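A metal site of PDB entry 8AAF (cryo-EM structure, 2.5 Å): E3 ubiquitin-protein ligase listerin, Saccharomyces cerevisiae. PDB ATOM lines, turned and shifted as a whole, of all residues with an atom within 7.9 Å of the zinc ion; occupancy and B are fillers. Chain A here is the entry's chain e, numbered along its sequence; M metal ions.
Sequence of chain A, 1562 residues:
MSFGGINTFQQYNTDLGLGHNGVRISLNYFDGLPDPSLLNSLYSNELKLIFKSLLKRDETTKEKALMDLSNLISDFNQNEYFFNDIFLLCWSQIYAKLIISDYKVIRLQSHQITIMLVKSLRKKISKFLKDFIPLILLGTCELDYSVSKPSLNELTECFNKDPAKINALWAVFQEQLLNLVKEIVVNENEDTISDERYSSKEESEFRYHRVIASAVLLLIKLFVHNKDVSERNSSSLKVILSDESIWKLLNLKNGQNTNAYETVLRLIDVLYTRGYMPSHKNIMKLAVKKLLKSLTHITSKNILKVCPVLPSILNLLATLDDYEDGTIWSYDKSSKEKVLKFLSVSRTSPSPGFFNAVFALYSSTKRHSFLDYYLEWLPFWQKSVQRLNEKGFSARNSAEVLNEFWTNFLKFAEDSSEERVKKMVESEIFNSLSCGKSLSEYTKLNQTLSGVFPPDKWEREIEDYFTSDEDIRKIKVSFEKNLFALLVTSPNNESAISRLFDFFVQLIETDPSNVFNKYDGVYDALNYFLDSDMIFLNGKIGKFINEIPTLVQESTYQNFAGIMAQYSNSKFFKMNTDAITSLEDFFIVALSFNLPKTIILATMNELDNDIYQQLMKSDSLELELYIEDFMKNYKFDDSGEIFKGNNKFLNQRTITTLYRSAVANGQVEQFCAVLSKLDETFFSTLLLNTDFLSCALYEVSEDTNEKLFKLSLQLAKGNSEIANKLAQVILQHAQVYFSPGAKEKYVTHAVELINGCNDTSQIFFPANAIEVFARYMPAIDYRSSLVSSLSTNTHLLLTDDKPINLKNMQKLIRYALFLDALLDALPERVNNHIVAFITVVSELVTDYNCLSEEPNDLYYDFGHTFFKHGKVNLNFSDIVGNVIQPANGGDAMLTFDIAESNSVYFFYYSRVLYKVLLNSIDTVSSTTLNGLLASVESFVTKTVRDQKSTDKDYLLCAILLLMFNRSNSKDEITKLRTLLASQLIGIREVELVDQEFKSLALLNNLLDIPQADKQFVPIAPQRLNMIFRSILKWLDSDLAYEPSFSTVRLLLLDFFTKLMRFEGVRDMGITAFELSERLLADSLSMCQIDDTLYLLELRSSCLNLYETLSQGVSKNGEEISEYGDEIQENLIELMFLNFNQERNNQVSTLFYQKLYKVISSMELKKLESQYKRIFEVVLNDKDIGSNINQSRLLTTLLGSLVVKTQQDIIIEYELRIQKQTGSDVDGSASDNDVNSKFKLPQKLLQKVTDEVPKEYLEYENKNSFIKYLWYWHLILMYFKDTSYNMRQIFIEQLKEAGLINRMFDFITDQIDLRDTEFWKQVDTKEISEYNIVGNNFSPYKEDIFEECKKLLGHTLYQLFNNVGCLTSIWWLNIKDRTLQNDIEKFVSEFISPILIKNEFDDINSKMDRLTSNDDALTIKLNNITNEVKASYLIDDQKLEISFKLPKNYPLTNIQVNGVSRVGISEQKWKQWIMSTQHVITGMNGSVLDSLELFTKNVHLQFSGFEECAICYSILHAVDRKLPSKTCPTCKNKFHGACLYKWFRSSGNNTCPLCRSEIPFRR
Within 4 Å of the zinc ion: Cys 1508, Cys 1511, His 1535 and Cys 1538.
The zinc ion is bound by ND1 of His 1535.
The side-chain sulfur (SG) of Cys 1511 is bound to the zinc ion, 2.3 Å away.
The zinc ion is bound by SG of Cys 1508 (2.3 Å).
The zinc ion is bound by the side-chain sulfur (SG) of Cys 1538 (2.3 Å).
The zinc ion has four donor atoms within binding distance.
NE2 of His 1535 lies within hydrogen-bond range of N of His 1516, at 3.3 Å.
A ring nitrogen (NE2) of His 1535 lies close to the backbone carbonyl oxygen (O) of Ser 1513, 3.3 Å away.
NE2 of His 1535 sits at hydrogen-bond distance from O of Ile 1514.
A ring nitrogen (NE2) of His 1535 sits close to the backbone carbonyl oxygen of Lys 1521, at 3.4 Å.
SG of Cys 1511 lies close to OG of Ser 1513, 3.0 Å away.
The side-chain sulfur (SG) of Cys 1508 lies close to the backbone NH (N) of Ile 1510.
N of Cys 1508 sits at hydrogen-bond distance from O of Ser 1513 (3.1 Å).
A ring nitrogen (NE2) of His 1516 sits close to the side-chain sulfur of Cys 1538 (3.6 Å).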
ATOM      1  N   GLU A1507      -0.802 -31.037  18.006  1.00  0.00           N
ATOM      2  CA  GLU A1507      -0.716 -29.593  17.830  1.00  0.00           C
ATOM      3  C   GLU A1507       0.689 -29.192  17.418  1.00  0.00           C
ATOM      4  O   GLU A1507       1.661 -29.832  17.809  1.00  0.00           O
ATOM      5  CB  GLU A1507      -1.101 -28.886  19.121  1.00  0.00           C
ATOM      6  CG  GLU A1507      -2.517 -29.174  19.574  1.00  0.00           C
ATOM      7  CD  GLU A1507      -2.871 -28.441  20.856  1.00  0.00           C
ATOM      8  OE1 GLU A1507      -1.952 -28.143  21.636  1.00  0.00           O
ATOM      9  OE2 GLU A1507      -4.073 -28.176  21.073  1.00  0.00           O
ATOM     10  N   CYS A1508       0.808 -28.115  16.641  1.00  0.00           N
ATOM     11  CA  CYS A1508       2.120 -27.629  16.263  1.00  0.00           C
ATOM     12  C   CYS A1508       2.879 -27.165  17.489  1.00  0.00           C
ATOM     13  O   CYS A1508       2.306 -26.505  18.346  1.00  0.00           O
ATOM     14  CB  CYS A1508       1.968 -26.484  15.280  1.00  0.00           C
ATOM     15  SG  CYS A1508       3.351 -25.341  15.141  1.00  0.00           S
ATOM     16  N   ALA A1509       4.153 -27.518  17.597  1.00  0.00           N
ATOM     17  CA  ALA A1509       4.913 -27.185  18.795  1.00  0.00           C
ATOM     18  C   ALA A1509       5.093 -25.692  19.017  1.00  0.00           C
ATOM     19  O   ALA A1509       4.971 -25.209  20.137  1.00  0.00           O
ATOM     20  CB  ALA A1509       6.255 -27.882  18.771  1.00  0.00           C
ATOM     21  N   ILE A1510       5.389 -24.946  17.951  1.00  0.00           N
ATOM     22  CA  ILE A1510       5.627 -23.517  18.096  1.00  0.00           C
ATOM     23  C   ILE A1510       4.395 -22.747  18.575  1.00  0.00           C
ATOM     24  O   ILE A1510       4.505 -21.904  19.462  1.00  0.00           O
ATOM     25  CB  ILE A1510       6.154 -22.912  16.782  1.00  0.00           C
ATOM     26  CG1 ILE A1510       7.357 -23.705  16.281  1.00  0.00           C
ATOM     27  CG2 ILE A1510       6.520 -21.446  16.952  1.00  0.00           C
ATOM     28  CD1 ILE A1510       8.019 -23.101  15.064  1.00  0.00           C
ATOM     29  N   CYS A1511       3.234 -23.039  18.009  1.00  0.00           N
ATOM     30  CA  CYS A1511       2.023 -22.291  18.369  1.00  0.00           C
ATOM     31  C   CYS A1511       0.990 -23.035  19.196  1.00  0.00           C
ATOM     32  O   CYS A1511      -0.048 -22.469  19.544  1.00  0.00           O
ATOM     33  CB  CYS A1511       1.374 -21.694  17.118  1.00  0.00           C
ATOM     34  SG  CYS A1511       0.752 -22.912  15.942  1.00  0.00           S
ATOM     35  N   TYR A1512       1.236 -24.308  19.491  1.00  0.00           N
ATOM     36  CA  TYR A1512       0.323 -25.105  20.317  1.00  0.00           C
ATOM     37  C   TYR A1512      -1.101 -25.160  19.787  1.00  0.00           C
ATOM     38  O   TYR A1512      -2.063 -25.127  20.558  1.00  0.00           O
ATOM     39  CB  TYR A1512       0.361 -24.659  21.789  1.00  0.00           C
ATOM     40  CG  TYR A1512       0.203 -25.787  22.776  1.00  0.00           C
ATOM     41  CD1 TYR A1512       1.085 -26.866  22.771  1.00  0.00           C
ATOM     42  CD2 TYR A1512      -0.812 -25.775  23.719  1.00  0.00           C
ATOM     43  CE1 TYR A1512       0.947 -27.898  23.676  1.00  0.00           C
ATOM     44  CE2 TYR A1512      -0.959 -26.812  24.627  1.00  0.00           C
ATOM     45  CZ  TYR A1512      -0.075 -27.864  24.599  1.00  0.00           C
ATOM     46  OH  TYR A1512      -0.216 -28.897  25.495  1.00  0.00           O
ATOM     47  N   SER A1513      -1.256 -25.221  18.471  1.00  0.00           N
ATOM     48  CA  SER A1513      -2.587 -25.336  17.874  1.00  0.00           C
ATOM     49  C   SER A1513      -2.545 -26.300  16.709  1.00  0.00           C
ATOM     50  O   SER A1513      -1.574 -26.332  15.967  1.00  0.00           O
ATOM     51  CB  SER A1513      -3.058 -23.963  17.390  1.00  0.00           C
ATOM     52  OG  SER A1513      -2.167 -23.430  16.423  1.00  0.00           O
ATOM     53  N   ILE A1514      -3.587 -27.102  16.553  1.00  0.00           N
ATOM     54  CA  ILE A1514      -3.655 -27.998  15.406  1.00  0.00           C
ATOM     55  C   ILE A1514      -3.766 -27.235  14.102  1.00  0.00           C
ATOM     56  O   ILE A1514      -3.167 -27.600  13.102  1.00  0.00           O
ATOM     57  CB  ILE A1514      -4.790 -29.020  15.533  1.00  0.00           C
ATOM     58  CG1 ILE A1514      -5.034 -29.381  17.008  1.00  0.00           C
ATOM     59  CG2 ILE A1514      -4.467 -30.278  14.756  1.00  0.00           C
ATOM     60  CD1 ILE A1514      -6.003 -30.529  17.196  1.00  0.00           C
ATOM     61  N   LEU A1515      -4.556 -26.156  14.102  1.00  0.00           N
ATOM     62  CA  LEU A1515      -4.756 -25.400  12.875  1.00  0.00           C
ATOM     63  C   LEU A1515      -4.060 -24.052  12.935  1.00  0.00           C
ATOM     64  O   LEU A1515      -4.227 -23.306  13.893  1.00  0.00           O
ATOM     65  CB  LEU A1515      -6.244 -25.210  12.594  1.00  0.00           C
ATOM     66  CG  LEU A1515      -7.032 -26.470  12.225  1.00  0.00           C
ATOM     67  CD1 LEU A1515      -8.523 -26.197  12.191  1.00  0.00           C
ATOM     68  CD2 LEU A1515      -6.554 -27.016  10.902  1.00  0.00           C
ATOM     69  N   HIS A1516      -3.277 -23.733  11.901  1.00  0.00           N
ATOM     70  CA  HIS A1516      -2.591 -22.446  11.861  1.00  0.00           C
ATOM     71  C   HIS A1516      -3.673 -21.402  11.800  1.00  0.00           C
ATOM     72  O   HIS A1516      -4.624 -21.529  11.055  1.00  0.00           O
ATOM     73  CB  HIS A1516      -1.717 -22.361  10.613  1.00  0.00           C
ATOM     74  CG  HIS A1516      -0.684 -21.285  10.668  1.00  0.00           C
ATOM     75  ND1 HIS A1516      -0.922 -19.994  10.235  1.00  0.00           N
ATOM     76  CD2 HIS A1516       0.597 -21.310  11.086  1.00  0.00           C
ATOM     77  CE1 HIS A1516       0.165 -19.271  10.402  1.00  0.00           C
ATOM     78  NE2 HIS A1516       1.117 -20.047  10.918  1.00  0.00           N
ATOM     79  N   ALA A1517      -3.557 -20.347  12.606  1.00  0.00           N
ATOM     80  CA  ALA A1517      -4.631 -19.375  12.638  1.00  0.00           C
ATOM     81  C   ALA A1517      -4.802 -18.672  11.301  1.00  0.00           C
ATOM     82  O   ALA A1517      -5.916 -18.536  10.811  1.00  0.00           O
ATOM     83  CB  ALA A1517      -4.393 -18.359  13.743  1.00  0.00           C
ATOM     84  N   LYS A1521      -4.491 -24.624   8.583  1.00  0.00           N
ATOM     85  CA  LYS A1521      -3.910 -25.889   8.108  1.00  0.00           C
ATOM     86  C   LYS A1521      -3.306 -26.759   9.203  1.00  0.00           C
ATOM     87  O   LYS A1521      -2.812 -26.255  10.201  1.00  0.00           O
ATOM     88  CB  LYS A1521      -2.853 -25.610   7.029  1.00  0.00           C
ATOM     89  CG  LYS A1521      -2.526 -26.812   6.166  1.00  0.00           C
ATOM     90  CD  LYS A1521      -1.204 -26.619   5.431  1.00  0.00           C
ATOM     91  CE  LYS A1521      -0.811 -27.881   4.686  1.00  0.00           C
ATOM     92  NZ  LYS A1521       0.520 -27.747   4.034  1.00  0.00           N
ATOM     93  N   PRO A1523      -0.597 -29.363  11.029  1.00  0.00           N
ATOM     94  CA  PRO A1523       0.854 -29.191  10.996  1.00  0.00           C
ATOM     95  C   PRO A1523       1.540 -30.296  10.215  1.00  0.00           C
ATOM     96  O   PRO A1523       1.855 -31.341  10.785  1.00  0.00           O
ATOM     97  CB  PRO A1523       1.255 -29.285  12.477  1.00  0.00           C
ATOM     98  CG  PRO A1523      -0.022 -29.226  13.253  1.00  0.00           C
ATOM     99  CD  PRO A1523      -1.061 -29.793  12.350  1.00  0.00           C
ATOM    100  N   LYS A1533       5.209 -31.891  15.728  1.00  0.00           N
ATOM    101  CA  LYS A1533       4.756 -31.438  14.417  1.00  0.00           C
ATOM    102  C   LYS A1533       4.710 -29.924  14.348  1.00  0.00           C
ATOM    103  O   LYS A1533       4.189 -29.289  15.254  1.00  0.00           O
ATOM    104  CB  LYS A1533       3.354 -31.978  14.135  1.00  0.00           C
ATOM    105  CG  LYS A1533       3.259 -33.498  14.036  1.00  0.00           C
ATOM    106  CD  LYS A1533       1.831 -33.917  13.758  1.00  0.00           C
ATOM    107  CE  LYS A1533       1.694 -35.431  13.723  1.00  0.00           C
ATOM    108  NZ  LYS A1533       0.267 -35.861  13.664  1.00  0.00           N
ATOM    109  N   PHE A1534       5.248 -29.351  13.282  1.00  0.00           N
ATOM    110  CA  PHE A1534       5.302 -27.905  13.156  1.00  0.00           C
ATOM    111  C   PHE A1534       4.547 -27.452  11.930  1.00  0.00           C
ATOM    112  O   PHE A1534       4.605 -28.098  10.895  1.00  0.00           O
ATOM    113  CB  PHE A1534       6.747 -27.434  13.001  1.00  0.00           C
ATOM    114  CG  PHE A1534       7.681 -27.918  14.073  1.00  0.00           C
ATOM    115  CD1 PHE A1534       7.807 -27.244  15.263  1.00  0.00           C
ATOM    116  CD2 PHE A1534       8.451 -29.053  13.872  1.00  0.00           C
ATOM    117  CE1 PHE A1534       8.670 -27.687  16.250  1.00  0.00           C
ATOM    118  CE2 PHE A1534       9.308 -29.509  14.851  1.00  0.00           C
ATOM    119  CZ  PHE A1534       9.416 -28.822  16.045  1.00  0.00           C
ATOM    120  N   HIS A1535       3.808 -26.347  12.030  1.00  0.00           N
ATOM    121  CA  HIS A1535       3.163 -25.811  10.843  1.00  0.00           C
ATOM    122  C   HIS A1535       4.304 -25.368   9.974  1.00  0.00           C
ATOM    123  O   HIS A1535       5.325 -24.891  10.469  1.00  0.00           O
ATOM    124  CB  HIS A1535       2.302 -24.597  11.150  1.00  0.00           C
ATOM    125  CG  HIS A1535       1.109 -24.885  11.997  1.00  0.00           C
ATOM    126  ND1 HIS A1535       0.891 -24.257  13.202  1.00  0.00           N
ATOM    127  CD2 HIS A1535       0.056 -25.711  11.803  1.00  0.00           C
ATOM    128  CE1 HIS A1535      -0.244 -24.693  13.715  1.00  0.00           C
ATOM    129  NE2 HIS A1535      -0.771 -25.577  12.885  1.00  0.00           N
ATOM    130  N   GLY A1536       4.150 -25.496   8.660  1.00  0.00           N
ATOM    131  CA  GLY A1536       5.240 -25.143   7.777  1.00  0.00           C
ATOM    132  C   GLY A1536       5.612 -23.692   7.904  1.00  0.00           C
ATOM    133  O   GLY A1536       6.785 -23.362   7.956  1.00  0.00           O
ATOM    134  N   ALA A1537       4.617 -22.822   7.991  1.00  0.00           N
ATOM    135  CA  ALA A1537       4.877 -21.389   8.098  1.00  0.00           C
ATOM    136  C   ALA A1537       5.619 -21.040   9.384  1.00  0.00           C
ATOM    137  O   ALA A1537       6.578 -20.258   9.346  1.00  0.00           O
ATOM    138  CB  ALA A1537       3.581 -20.615   8.023  1.00  0.00           C
ATOM    139  N   CYS A1538       5.214 -21.633  10.506  1.00  0.00           N
ATOM    140  CA  CYS A1538       5.891 -21.356  11.761  1.00  0.00           C
ATOM    141  C   CYS A1538       7.332 -21.834  11.701  1.00  0.00           C
ATOM    142  O   CYS A1538       8.238 -21.140  12.149  1.00  0.00           O
ATOM    143  CB  CYS A1538       5.182 -22.066  12.911  1.00  0.00           C
ATOM    144  SG  CYS A1538       3.456 -21.595  13.208  1.00  0.00           S
ATOM    145  N   LEU A1539       7.540 -23.015  11.141  1.00  0.00           N
ATOM    146  CA  LEU A1539       8.889 -23.570  11.069  1.00  0.00           C
ATOM    147  C   LEU A1539       9.790 -22.707  10.202  1.00  0.00           C
ATOM    148  O   LEU A1539      10.927 -22.439  10.568  1.00  0.00           O
ATOM    149  CB  LEU A1539       8.841 -24.985  10.495  1.00  0.00           C
ATOM    150  CG  LEU A1539      10.106 -25.815  10.643  1.00  0.00           C
ATOM    151  CD1 LEU A1539      10.443 -25.972  12.113  1.00  0.00           C
ATOM    152  CD2 LEU A1539       9.931 -27.170   9.979  1.00  0.00           C
HETATM  153 ZN    ZN M   1       2.411 -23.349  14.353  1.00  0.00          ZN
